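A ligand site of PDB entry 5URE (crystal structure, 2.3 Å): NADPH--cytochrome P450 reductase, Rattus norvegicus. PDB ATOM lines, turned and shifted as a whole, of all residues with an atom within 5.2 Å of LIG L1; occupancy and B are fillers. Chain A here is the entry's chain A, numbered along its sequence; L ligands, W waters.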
ATOM      1  N   ARG A 242      -4.295   6.274  33.485  1.00  0.00           N
ATOM      2  CA  ARG A 242      -3.890   7.460  34.233  1.00  0.00           C
ATOM      3  C   ARG A 242      -5.098   8.371  34.354  1.00  0.00           C
ATOM      4  O   ARG A 242      -6.202   8.011  33.920  1.00  0.00           O
ATOM      5  CB  ARG A 242      -2.777   8.186  33.495  1.00  0.00           C
ATOM      6  CG  ARG A 242      -1.609   7.305  33.101  1.00  0.00           C
ATOM      7  CD  ARG A 242      -1.025   7.765  31.770  1.00  0.00           C
ATOM      8  NE  ARG A 242      -0.037   8.822  31.910  1.00  0.00           N
ATOM      9  CZ  ARG A 242       0.182   9.766  31.000  1.00  0.00           C
ATOM     10  NH1 ARG A 242      -0.529   9.787  29.876  1.00  0.00           N
ATOM     11  NH2 ARG A 242       1.125  10.668  31.208  1.00  0.00           N
ATOM     12  N   VAL A 418      -1.816  16.192  34.229  1.00  0.00           N
ATOM     13  CA  VAL A 418      -1.920  14.773  34.520  1.00  0.00           C
ATOM     14  C   VAL A 418      -1.682  14.622  36.014  1.00  0.00           C
ATOM     15  O   VAL A 418      -0.731  15.196  36.547  1.00  0.00           O
ATOM     16  CB  VAL A 418      -0.861  13.928  33.732  1.00  0.00           C
ATOM     17  CG1 VAL A 418       0.540  14.470  33.958  1.00  0.00           C
ATOM     18  CG2 VAL A 418      -0.941  12.460  34.177  1.00  0.00           C
ATOM     19  N   PRO A 477       3.672  16.947  22.658  1.00  0.00           N
ATOM     20  CA  PRO A 477       3.126  15.624  22.996  1.00  0.00           C
ATOM     21  C   PRO A 477       2.644  15.534  24.448  1.00  0.00           C
ATOM     22  O   PRO A 477       3.182  16.176  25.344  1.00  0.00           O
ATOM     23  CB  PRO A 477       4.298  14.696  22.706  1.00  0.00           C
ATOM     24  CG  PRO A 477       5.484  15.555  23.058  1.00  0.00           C
ATOM     25  CD  PRO A 477       5.120  16.869  22.397  1.00  0.00           C
ATOM     26  N   GLY A 478       1.607  14.723  24.663  1.00  0.00           N
ATOM     27  CA  GLY A 478       1.054  14.558  25.992  1.00  0.00           C
ATOM     28  C   GLY A 478       0.457  15.841  26.514  1.00  0.00           C
ATOM     29  O   GLY A 478      -0.228  16.559  25.766  1.00  0.00           O
ATOM     30  N   THR A 479       0.732  16.152  27.778  1.00  0.00           N
ATOM     31  CA  THR A 479       0.200  17.370  28.384  1.00  0.00           C
ATOM     32  C   THR A 479       0.908  18.605  27.830  1.00  0.00           C
ATOM     33  O   THR A 479       0.510  19.744  28.097  1.00  0.00           O
ATOM     34  CB  THR A 479       0.364  17.352  29.929  1.00  0.00           C
ATOM     35  OG1 THR A 479       1.746  17.352  30.263  1.00  0.00           O
ATOM     36  CG2 THR A 479      -0.283  16.103  30.507  1.00  0.00           C
ATOM     37  N   GLY A 480       1.956  18.379  27.040  1.00  0.00           N
ATOM     38  CA  GLY A 480       2.666  19.499  26.466  1.00  0.00           C
ATOM     39  C   GLY A 480       1.775  20.287  25.517  1.00  0.00           C
ATOM     40  O   GLY A 480       2.126  21.359  25.047  1.00  0.00           O
ATOM     41  N   GLY A 509       1.140  14.213  20.324  1.00  0.00           N
ATOM     42  CA  GLY A 509       1.399  12.805  20.494  1.00  0.00           C
ATOM     43  C   GLY A 509       0.815  12.250  21.784  1.00  0.00           C
ATOM     44  O   GLY A 509       0.817  12.901  22.830  1.00  0.00           O
ATOM     45  N   CYS A 510       0.284  11.035  21.702  1.00  0.00           N
ATOM     46  CA  CYS A 510      -0.259  10.381  22.865  1.00  0.00           C
ATOM     47  C   CYS A 510       0.062   8.895  22.716  1.00  0.00           C
ATOM     48  O   CYS A 510       0.756   8.507  21.776  1.00  0.00           O
ATOM     49  CB  CYS A 510      -1.771  10.617  22.963  1.00  0.00           C
ATOM     50  SG  CYS A 510      -2.720  10.040  21.536  1.00  0.00           S
ATOM     51  N   ARG A 511      -0.430   8.075  23.632  1.00  0.00           N
ATOM     52  CA  ARG A 511      -0.157   6.650  23.577  1.00  0.00           C
ATOM     53  C   ARG A 511      -1.118   5.927  22.630  1.00  0.00           C
ATOM     54  O   ARG A 511      -0.680   5.290  21.669  1.00  0.00           O
ATOM     55  CB  ARG A 511      -0.228   6.077  24.985  1.00  0.00           C
ATOM     56  CG  ARG A 511       0.680   6.832  25.949  1.00  0.00           C
ATOM     57  CD  ARG A 511       0.659   6.257  27.366  1.00  0.00           C
ATOM     58  NE  ARG A 511       1.557   7.017  28.230  1.00  0.00           N
ATOM     59  CZ  ARG A 511       1.822   6.715  29.503  1.00  0.00           C
ATOM     60  NH1 ARG A 511       1.258   5.651  30.060  1.00  0.00           N
ATOM     61  NH2 ARG A 511       2.663   7.469  30.196  1.00  0.00           N
ATOM     62  N   ASP A 516      -5.560   8.033  25.849  1.00  0.00           N
ATOM     63  CA  ASP A 516      -5.228   9.381  26.320  1.00  0.00           C
ATOM     64  C   ASP A 516      -5.061  10.462  25.242  1.00  0.00           C
ATOM     65  O   ASP A 516      -4.138  11.279  25.301  1.00  0.00           O
ATOM     66  CB  ASP A 516      -3.978   9.336  27.202  1.00  0.00           C
ATOM     67  CG  ASP A 516      -2.804   8.627  26.546  1.00  0.00           C
ATOM     68  OD1 ASP A 516      -2.758   8.526  25.292  1.00  0.00           O
ATOM     69  OD2 ASP A 516      -1.893   8.173  27.291  1.00  0.00           O
ATOM     70  N   ALA A 538       0.966  11.586  16.668  1.00  0.00           N
ATOM     71  CA  ALA A 538       1.768  10.377  16.783  1.00  0.00           C
ATOM     72  C   ALA A 538       1.239   9.499  17.902  1.00  0.00           C
ATOM     73  O   ALA A 538       1.275   9.893  19.069  1.00  0.00           O
ATOM     74  CB  ALA A 538       3.214  10.758  17.066  1.00  0.00           C
ATOM     75  N   SER A 540       2.091   6.737  20.019  1.00  0.00           N
ATOM     76  CA  SER A 540       3.268   5.972  20.390  1.00  0.00           C
ATOM     77  C   SER A 540       3.079   4.509  20.676  1.00  0.00           C
ATOM     78  O   SER A 540       4.023   3.728  20.539  1.00  0.00           O
ATOM     79  CB  SER A 540       3.961   6.633  21.592  1.00  0.00           C
ATOM     80  OG  SER A 540       3.232   6.427  22.793  1.00  0.00           O
ATOM     81  N   ARG A 541       1.871   4.078  21.041  1.00  0.00           N
ATOM     82  CA  ARG A 541       1.715   2.671  21.372  1.00  0.00           C
ATOM     83  C   ARG A 541       0.714   1.831  20.604  1.00  0.00           C
ATOM     84  O   ARG A 541       0.439   0.703  20.996  1.00  0.00           O
ATOM     85  CB  ARG A 541       1.427   2.555  22.880  1.00  0.00           C
ATOM     86  CG  ARG A 541       2.470   3.272  23.737  1.00  0.00           C
ATOM     87  CD  ARG A 541       2.217   3.101  25.222  1.00  0.00           C
ATOM     88  NE  ARG A 541       3.197   3.855  26.011  1.00  0.00           N
ATOM     89  CZ  ARG A 541       3.208   3.883  27.343  1.00  0.00           C
ATOM     90  NH1 ARG A 541       2.293   3.187  28.027  1.00  0.00           N
ATOM     91  NH2 ARG A 541       4.102   4.610  27.998  1.00  0.00           N
ATOM     92  N   LYS A 546       7.769   2.623  18.345  1.00  0.00           N
ATOM     93  CA  LYS A 546       7.371   3.930  18.847  1.00  0.00           C
ATOM     94  C   LYS A 546       7.178   4.899  17.699  1.00  0.00           C
ATOM     95  O   LYS A 546       7.946   4.880  16.737  1.00  0.00           O
ATOM     96  CB  LYS A 546       8.438   4.500  19.787  1.00  0.00           C
ATOM     97  CG  LYS A 546       8.636   3.752  21.094  1.00  0.00           C
ATOM     98  CD  LYS A 546       7.367   3.771  21.961  1.00  0.00           C
ATOM     99  CE  LYS A 546       7.650   3.179  23.328  1.00  0.00           C
ATOM    100  NZ  LYS A 546       6.462   3.186  24.218  1.00  0.00           N
ATOM    101  N   TYR A 548       6.811   8.922  17.384  1.00  0.00           N
ATOM    102  CA  TYR A 548       6.839  10.156  18.121  1.00  0.00           C
ATOM    103  C   TYR A 548       6.650  11.360  17.223  1.00  0.00           C
ATOM    104  O   TYR A 548       6.727  11.250  15.999  1.00  0.00           O
ATOM    105  CB  TYR A 548       8.163  10.293  18.875  1.00  0.00           C
ATOM    106  CG  TYR A 548       8.363   9.249  19.972  1.00  0.00           C
ATOM    107  CD1 TYR A 548       7.322   8.897  20.824  1.00  0.00           C
ATOM    108  CD2 TYR A 548       9.623   8.688  20.207  1.00  0.00           C
ATOM    109  CE1 TYR A 548       7.537   8.018  21.901  1.00  0.00           C
ATOM    110  CE2 TYR A 548       9.837   7.814  21.277  1.00  0.00           C
ATOM    111  CZ  TYR A 548       8.793   7.497  22.118  1.00  0.00           C
ATOM    112  OH  TYR A 548       9.019   6.699  23.224  1.00  0.00           O
ATOM    113  N   VAL A 549       6.397  12.506  17.841  1.00  0.00           N
ATOM    114  CA  VAL A 549       6.205  13.721  17.085  1.00  0.00           C
ATOM    115  C   VAL A 549       7.393  14.024  16.155  1.00  0.00           C
ATOM    116  O   VAL A 549       7.187  14.414  15.005  1.00  0.00           O
ATOM    117  CB  VAL A 549       5.944  14.908  18.025  1.00  0.00           C
ATOM    118  CG1 VAL A 549       4.562  14.774  18.653  1.00  0.00           C
ATOM    119  CG2 VAL A 549       7.010  14.961  19.108  1.00  0.00           C
ATOM    120  N   GLN A 550       8.623  13.821  16.616  1.00  0.00           N
ATOM    121  CA  GLN A 550       9.772  14.098  15.759  1.00  0.00           C
ATOM    122  C   GLN A 550       9.762  13.255  14.486  1.00  0.00           C
ATOM    123  O   GLN A 550      10.328  13.653  13.458  1.00  0.00           O
ATOM    124  CB  GLN A 550      11.117  13.928  16.489  1.00  0.00           C
ATOM    125  CG  GLN A 550      11.355  12.565  17.130  1.00  0.00           C
ATOM    126  CD  GLN A 550      10.820  12.510  18.550  1.00  0.00           C
ATOM    127  OE1 GLN A 550       9.766  13.060  18.866  1.00  0.00           O
ATOM    128  NE2 GLN A 550      11.560  11.830  19.430  1.00  0.00           N
ATOM    129  N   GLY A 575       6.515  20.671  26.734  1.00  0.00           N
ATOM    130  CA  GLY A 575       6.416  19.367  27.371  1.00  0.00           C
ATOM    131  C   GLY A 575       7.704  18.961  28.063  1.00  0.00           C
ATOM    132  O   GLY A 575       8.419  19.785  28.627  1.00  0.00           O
ATOM    133  N   ASP A 576       7.985  17.665  28.011  1.00  0.00           N
ATOM    134  CA  ASP A 576       9.171  17.078  28.623  1.00  0.00           C
ATOM    135  C   ASP A 576      10.481  17.710  28.159  1.00  0.00           C
ATOM    136  O   ASP A 576      10.814  17.644  26.979  1.00  0.00           O
ATOM    137  CB  ASP A 576       9.205  15.566  28.329  1.00  0.00           C
ATOM    138  CG  ASP A 576      10.531  14.918  28.736  1.00  0.00           C
ATOM    139  OD1 ASP A 576      10.907  15.033  29.919  1.00  0.00           O
ATOM    140  OD2 ASP A 576      11.197  14.299  27.878  1.00  0.00           O
ATOM    141  N   ASN A 579      13.966  14.583  27.579  1.00  0.00           N
ATOM    142  CA  ASN A 579      14.311  13.906  26.329  1.00  0.00           C
ATOM    143  C   ASN A 579      13.604  14.403  25.095  1.00  0.00           C
ATOM    144  O   ASN A 579      14.226  14.540  24.040  1.00  0.00           O
ATOM    145  CB  ASN A 579      14.079  12.387  26.427  1.00  0.00           C
ATOM    146  CG  ASN A 579      15.134  11.682  27.237  1.00  0.00           C
ATOM    147  OD1 ASN A 579      14.945  11.414  28.426  1.00  0.00           O
ATOM    148  ND2 ASN A 579      16.267  11.385  26.618  1.00  0.00           N
ATOM    149  N   MET A 580      12.310  14.656  25.218  1.00  0.00           N
ATOM    150  CA  MET A 580      11.506  15.102  24.079  1.00  0.00           C
ATOM    151  C   MET A 580      12.021  16.373  23.411  1.00  0.00           C
ATOM    152  O   MET A 580      12.183  16.415  22.190  1.00  0.00           O
ATOM    153  CB  MET A 580      10.047  15.266  24.518  1.00  0.00           C
ATOM    154  CG  MET A 580       9.097  15.663  23.401  1.00  0.00           C
ATOM    155  SD  MET A 580       9.178  17.426  22.996  1.00  0.00           S
ATOM    156  CE  MET A 580       8.327  18.118  24.426  1.00  0.00           C
ATOM    157  N   ASP A 583      15.228  15.711  21.431  1.00  0.00           N
ATOM    158  CA  ASP A 583      14.986  14.863  20.275  1.00  0.00           C
ATOM    159  C   ASP A 583      14.361  15.721  19.170  1.00  0.00           C
ATOM    160  O   ASP A 583      14.791  15.687  18.011  1.00  0.00           O
ATOM    161  CB  ASP A 583      14.052  13.702  20.635  1.00  0.00           C
ATOM    162  CG  ASP A 583      14.768  12.567  21.381  1.00  0.00           C
ATOM    163  OD1 ASP A 583      16.016  12.550  21.408  1.00  0.00           O
ATOM    164  OD2 ASP A 583      14.076  11.683  21.943  1.00  0.00           O
ATOM    165  N   TRP A 621       9.241  21.438  30.801  1.00  0.00           N
ATOM    166  CA  TRP A 621       9.193  21.234  32.243  1.00  0.00           C
ATOM    167  C   TRP A 621      10.103  20.198  32.851  1.00  0.00           C
ATOM    168  O   TRP A 621      10.471  19.205  32.223  1.00  0.00           O
ATOM    169  CB  TRP A 621       7.760  20.943  32.677  1.00  0.00           C
ATOM    170  CG  TRP A 621       6.733  21.664  31.852  1.00  0.00           C
ATOM    171  CD1 TRP A 621       6.779  22.967  31.441  1.00  0.00           C
ATOM    172  CD2 TRP A 621       5.517  21.129  31.331  1.00  0.00           C
ATOM    173  NE1 TRP A 621       5.673  23.273  30.691  1.00  0.00           N
ATOM    174  CE2 TRP A 621       4.870  22.160  30.609  1.00  0.00           C
ATOM    175  CE3 TRP A 621       4.897  19.877  31.406  1.00  0.00           C
ATOM    176  CZ2 TRP A 621       3.651  21.971  29.960  1.00  0.00           C
ATOM    177  CZ3 TRP A 621       3.677  19.695  30.764  1.00  0.00           C
ATOM    178  CH2 TRP A 621       3.080  20.732  30.057  1.00  0.00           C
ATOM    179  N   SER A 622      10.424  20.443  34.122  1.00  0.00           N
ATOM    180  CA  SER A 622      11.265  19.574  34.927  1.00  0.00           C
ATOM    181  C   SER A 622      10.878  19.844  36.387  1.00  0.00           C
ATOM    182  O   SER A 622      10.051  20.745  36.630  1.00  0.00           O
ATOM    183  CB  SER A 622      12.738  19.944  34.715  1.00  0.00           C
ATOM    184  OG  SER A 622      12.983  21.252  35.223  1.00  0.00           O
ATOM    185  OXT SER A 622      11.410  19.130  37.280  1.00  0.00           O
HETATM  186  P1  LIG L   1       3.179  10.798  28.303  1.00  0.00           P
HETATM  187  O1  LIG L   1       2.044   9.933  27.917  1.00  0.00           O
HETATM  188  O2  LIG L   1       4.107  10.322  29.354  1.00  0.00           O
HETATM  189  O3  LIG L   1       4.011  11.191  26.989  1.00  0.00           O
HETATM  190  C1  LIG L   1       3.303  11.777  25.883  1.00  0.00           C
HETATM  191  C2  LIG L   1       3.802  11.174  24.566  1.00  0.00           C
HETATM  192  O4  LIG L   1       5.203  11.449  24.410  1.00  0.00           O
HETATM  193  C3  LIG L   1       3.661   9.658  24.595  1.00  0.00           C
HETATM  194  O5  LIG L   1       3.189   9.211  23.309  1.00  0.00           O
HETATM  195  C4  LIG L   1       5.092   9.190  24.819  1.00  0.00           C
HETATM  196  O6  LIG L   1       5.269   7.884  24.256  1.00  0.00           O
HETATM  197  C5  LIG L   1       5.784  10.219  23.948  1.00  0.00           C
HETATM  198  N1  LIG L   1       7.257  10.248  24.090  1.00  0.00           N
HETATM  199  C6  LIG L   1       7.980   9.628  25.021  1.00  0.00           C
HETATM  200  N2  LIG L   1       9.244   9.980  24.848  1.00  0.00           N
HETATM  201  C7  LIG L   1       9.315  10.806  23.810  1.00  0.00           C
HETATM  202  C8  LIG L   1      10.349  11.400  23.215  1.00  0.00           C
HETATM  203  N3  LIG L   1      11.562  10.981  23.587  1.00  0.00           N
HETATM  204  N4  LIG L   1      10.191  12.209  22.167  1.00  0.00           N
HETATM  205  C9  LIG L   1       8.906  12.463  21.686  1.00  0.00           C
HETATM  206  N5  LIG L   1       7.836  11.820  22.334  1.00  0.00           N
HETATM  207  C10 LIG L   1       8.076  10.996  23.364  1.00  0.00           C
HETATM  208  O7  LIG L   1       2.589  12.219  28.770  1.00  0.00           O
HETATM  209  P2  LIG L   1       2.898  13.302  29.923  1.00  0.00           P
HETATM  210  O8  LIG L   1       2.306  12.829  31.191  1.00  0.00           O
HETATM  211  O9  LIG L   1       2.521  14.633  29.409  1.00  0.00           O
HETATM  212  O10 LIG L   1       4.494  13.208  30.070  1.00  0.00           O
HETATM  213  C11 LIG L   1       5.338  13.258  28.913  1.00  0.00           C
HETATM  214  C12 LIG L   1       6.789  13.466  29.338  1.00  0.00           C
HETATM  215  O11 LIG L   1       6.876  14.717  30.046  1.00  0.00           O
HETATM  216  C13 LIG L   1       7.204  12.400  30.335  1.00  0.00           C
HETATM  217  O12 LIG L   1       8.617  12.154  30.249  1.00  0.00           O
HETATM  218  C14 LIG L   1       6.890  13.071  31.657  1.00  0.00           C
HETATM  219  O13 LIG L   1       7.650  12.471  32.708  1.00  0.00           O
HETATM  220  C15 LIG L   1       7.471  14.434  31.323  1.00  0.00           C
HETATM  221  N6  LIG L   1       7.175  15.466  32.333  1.00  0.00           N
HETATM  222  C16 LIG L   1       5.857  15.850  32.593  1.00  0.00           C
HETATM  223  C17 LIG L   1       5.582  16.757  33.613  1.00  0.00           C
HETATM  224  C18 LIG L   1       4.264  17.152  33.844  1.00  0.00           C
HETATM  225  O14 LIG L   1       3.425  17.107  32.936  1.00  0.00           O
HETATM  226  N7  LIG L   1       4.049  17.742  35.012  1.00  0.00           N
HETATM  227  C19 LIG L   1       6.617  17.273  34.380  1.00  0.00           C
HETATM  228  C20 LIG L   1       7.932  16.917  34.117  1.00  0.00           C
HETATM  229  C21 LIG L   1       8.215  16.019  33.104  1.00  0.00           C
HETATM  230  P3  LIG L   1       5.617   6.605  25.170  1.00  0.00           P
HETATM  231  O15 LIG L   1       5.217   7.009  26.547  1.00  0.00           O
HETATM  232  O16 LIG L   1       7.075   6.413  24.996  1.00  0.00           O
HETATM  233  O17 LIG L   1       4.776   5.532  24.587  1.00  0.00           O
HETATM  234  P1  LG2 L   2       4.627  17.047  43.305  1.00  0.00           P
HETATM  235  O1  LG2 L   2       4.080  16.625  44.613  1.00  0.00           O
HETATM  236  O2  LG2 L   2       5.166  18.415  43.162  1.00  0.00           O
HETATM  237  O3  LG2 L   2       5.744  15.980  42.863  1.00  0.00           O
HETATM  238  C1  LG2 L   2       6.532  16.187  41.684  1.00  0.00           C
HETATM  239  C2  LG2 L   2       7.705  15.206  41.704  1.00  0.00           C
HETATM  240  O4  LG2 L   2       7.257  13.844  41.806  1.00  0.00           O
HETATM  241  C3  LG2 L   2       8.436  15.203  40.378  1.00  0.00           C
HETATM  242  O5  LG2 L   2       9.286  16.365  40.315  1.00  0.00           O
HETATM  243  C4  LG2 L   2       9.299  13.974  40.603  1.00  0.00           C
HETATM  244  O6  LG2 L   2      10.392  14.298  41.479  1.00  0.00           O
HETATM  245  C5  LG2 L   2       8.340  13.026  41.313  1.00  0.00           C
HETATM  246  N1  LG2 L   2       7.746  12.041  40.381  1.00  0.00           N
HETATM  247  C6  LG2 L   2       6.658  12.294  39.415  1.00  0.00           C
HETATM  248  N2  LG2 L   2       6.449  10.925  38.891  1.00  0.00           N
HETATM  249  C7  LG2 L   2       7.357  10.119  39.430  1.00  0.00           C
HETATM  250  C8  LG2 L   2       7.540   8.809  39.243  1.00  0.00           C
HETATM  251  N3  LG2 L   2       6.607   8.186  38.522  1.00  0.00           N
HETATM  252  N4  LG2 L   2       8.536   8.129  39.830  1.00  0.00           N
HETATM  253  C9  LG2 L   2       9.411   8.814  40.672  1.00  0.00           C
HETATM  254  N5  LG2 L   2       9.202  10.184  40.847  1.00  0.00           N
HETATM  255  C10 LG2 L   2       8.184  10.795  40.229  1.00  0.00           C
HETATM  256  N6  LG2 L   2       2.373  19.930  34.252  1.00  0.00           N
HETATM  257  C11 LG2 L   2       1.175  19.629  33.599  1.00  0.00           C
HETATM  258  O7  LG2 L   2       0.594  18.573  33.850  1.00  0.00           O
HETATM  259  N7  LG2 L   2       0.600  20.570  32.743  1.00  0.00           N
HETATM  260  C12 LG2 L   2       1.202  21.811  32.555  1.00  0.00           C
HETATM  261  O8  LG2 L   2       0.622  22.676  31.897  1.00  0.00           O
HETATM  262  C13 LG2 L   2       2.378  22.126  33.221  1.00  0.00           C
HETATM  263  N8  LG2 L   2       3.066  23.230  32.911  1.00  0.00           N
HETATM  264  C14 LG2 L   2       4.194  23.526  33.577  1.00  0.00           C
HETATM  265  C15 LG2 L   2       4.895  24.697  33.283  1.00  0.00           C
HETATM  266  C16 LG2 L   2       6.062  24.999  33.978  1.00  0.00           C
HETATM  267  C17 LG2 L   2       6.719  26.205  33.730  1.00  0.00           C
HETATM  268  C18 LG2 L   2       6.538  24.137  34.960  1.00  0.00           C
HETATM  269  C19 LG2 L   2       7.695  24.438  35.654  1.00  0.00           C
HETATM  270  C20 LG2 L   2       5.814  22.987  35.273  1.00  0.00           C
HETATM  271  C21 LG2 L   2       4.636  22.694  34.612  1.00  0.00           C
HETATM  272  N9  LG2 L   2       3.939  21.580  34.902  1.00  0.00           N
HETATM  273  C22 LG2 L   2       2.974  21.186  34.062  1.00  0.00           C
HETATM  274  C23 LG2 L   2       4.325  20.699  36.018  1.00  0.00           C
HETATM  275  C24 LG2 L   2       3.597  21.182  37.276  1.00  0.00           C
HETATM  276  O9  LG2 L   2       4.055  22.489  37.612  1.00  0.00           O
HETATM  277  C25 LG2 L   2       3.814  20.263  38.477  1.00  0.00           C
HETATM  278  O10 LG2 L   2       5.216  20.087  38.726  1.00  0.00           O
HETATM  279  C26 LG2 L   2       3.138  18.909  38.261  1.00  0.00           C
HETATM  280  O11 LG2 L   2       1.745  19.102  38.039  1.00  0.00           O
HETATM  281  C27 LG2 L   2       3.349  18.043  39.507  1.00  0.00           C
HETATM  282  O12 LG2 L   2       2.873  18.741  40.654  1.00  0.00           O
HETATM  283  P2  LG2 L   2       2.334  17.940  41.943  1.00  0.00           P
HETATM  284  O13 LG2 L   2       1.082  17.243  41.562  1.00  0.00           O
HETATM  285  O14 LG2 L   2       2.296  18.875  43.100  1.00  0.00           O
HETATM  286  O15 LG2 L   2       3.476  16.834  42.199  1.00  0.00           O
HETATM  287  O   HOH W   1       1.095  17.154  36.404  1.00  0.00           O
HETATM  288  O   HOH W   2       9.174  12.628  26.993  1.00  0.00           O
HETATM  289  O   HOH W   3       6.948  13.343  25.647  1.00  0.00           O
HETATM  290  O   HOH W   4       3.546  15.582  36.200  1.00  0.00           O
HETATM  291  O   HOH W   5       0.016  10.215  26.269  1.00  0.00           O
HETATM  292  O   HOH W   6      11.954  11.848  29.478  1.00  0.00           O
HETATM  293  O   HOH W   7       5.078  10.054  31.823  1.00  0.00           O
HETATM  294  O   HOH W   8       6.340   8.719  28.354  1.00  0.00           O
HETATM  295  O   HOH W   9       5.628  12.202  20.653  1.00  0.00           O
HETATM  296  O   HOH W  10       5.991  16.018  27.040  1.00  0.00           O
HETATM  297  O   HOH W  11       3.590  10.247  20.827  1.00  0.00           O
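Val 418 touches LIG L1 (CG1 to O8, 3.7 Å). Pro 477 touches LIG L1 (CB to O4, 3.8 Å). CA of Gly 478 touches C1 of LIG L1, at 3.6 Å. O of Gly 509 touches C2 of LIG L1, at 3.9 Å. Asp 576 touches LIG L1. Met 580 touches LIG L1. Trp 621 touches LIG L1 (CZ3 to O14, 3.4 Å). Hydrophobic or aromatic side chains within 4 Å of LIG L1: Val 418, Pro 477, Tyr 548, Met 580 and Trp 621. Within 4 Å of LIG L1: Arg 242, Val 418, Pro 477, Gly 478, Thr 479, Gly 509, Cys 510, Arg 511, Ser 540, Arg 541, Lys 546, Tyr 548, Gln 550, Asp 576, Met 580, Asp 583 and Trp 621. The nearest printed residue that does not touch LIG L1 is Asn 579 (4.05 Å).
Water W5 lies within hydrogen-bond range of O1 of LIG L1 (2.6 Å), OD2 of Asp 516 (3.0 Å) and N of Arg 511 (3.4 Å). Water W11 lies within hydrogen-bond range of an oxygen (O5) of LIG L1 (2.7 Å), the backbone carbonyl oxygen of Ala 538 (2.9 Å) and the backbone carbonyl oxygen of Cys 510 (3.5 Å). Water W9 bridges N5 of LIG L1 (2.8 Å) and N of Val 549 (2.9 Å). Water W1 lies within hydrogen-bond range of O11 of LG2 L2 (2.6 Å), O of Val 418 (2.7 Å) and N7 of LIG L1 (3.3 Å). Water W2 lies within hydrogen-bond range of the side-chain carboxylate (OD2) of Asp 576 (2.8 Å) and an oxygen (O12) of LIG L1 (3.3 Å). Water W10 lies within hydrogen-bond range of the backbone NH (N) of Asp 576 (2.8 Å), the backbone carbonyl oxygen (O) of Pro 477 (3.3 Å) and an oxygen (O11) of LIG L1 (3.4 Å).
OD2 of Asp 576 sits at hydrogen-bond distance from N of Met 580, at 2.9 Å. The guanidinium group of Arg 242 is in salt-bridge range of the side-chain carboxylate of Asp 516, 3.3 Å away. The backbone carbonyl oxygen (O) of Gly 575 lies within hydrogen-bond range of the backbone NH (N) of Trp 621 (2.9 Å). The backbone NH (N) of Ser 540 lies within hydrogen-bond range of the backbone carbonyl oxygen (O) of Cys 510 (2.8 Å). The backbone NH (N) of Cys 510 lies within hydrogen-bond range of the backbone carbonyl oxygen (O) of Ala 538. O of Gly 509 lies within hydrogen-bond range of N of Gly 478 (2.7 Å). NE of Arg 511 is in salt-bridge range of OD2 of Asp 516. The backbone NH of Arg 541 sits at hydrogen-bond distance from the backbone carbonyl oxygen of Arg 511.
N6 of LG2 L2 is in hydrogen-bond range of N7 of LIG L1 (2.9 Å).
O16 of LIG L1 is in hydrogen-bond range of OH of Tyr 548 (2.6 Å). A nitrogen (N3) of LIG L1 sits at hydrogen-bond distance from the side-chain carboxylate (OD2) of Asp 583 (3.1 Å). O9 of LIG L1 sits at hydrogen-bond distance from N of Thr 479 (2.9 Å). N8 of LG2 L2 lies close to NE1 of Trp 621, 3.4 Å away. NE2 of Gln 550 lies within hydrogen-bond range of N4 of LIG L1 (3.1 Å). N of Val 418 lies within hydrogen-bond range of O7 of LG2 L2, 3.4 Å away. An oxygen (O5) of LIG L1 lies within hydrogen-bond range of the backbone carbonyl oxygen (O) of Cys 510, at 3.0 Å. The side-chain amino group (NZ) of Lys 546 lies within salt-bridge range of an oxygen (O17) of LIG L1, at 2.9 Å. The guanidinium group (NE) of Arg 511 lies within salt-bridge range of an oxygen (O1) of LIG L1 (3.0 Å). O9 of LIG L1 sits at hydrogen-bond distance from OG1 of Thr 479, at 3.0 Å. An oxygen (O8) of LIG L1 is in salt-bridge range of the guanidinium group (NH2) of Arg 242, at 2.5 Å. NE of Arg 541 lies within salt-bridge range of O17 of LIG L1 (2.7 Å). The side-chain hydroxyl of Ser 540 sits at hydrogen-bond distance from an oxygen (O17) of LIG L1, 2.5 Å away.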
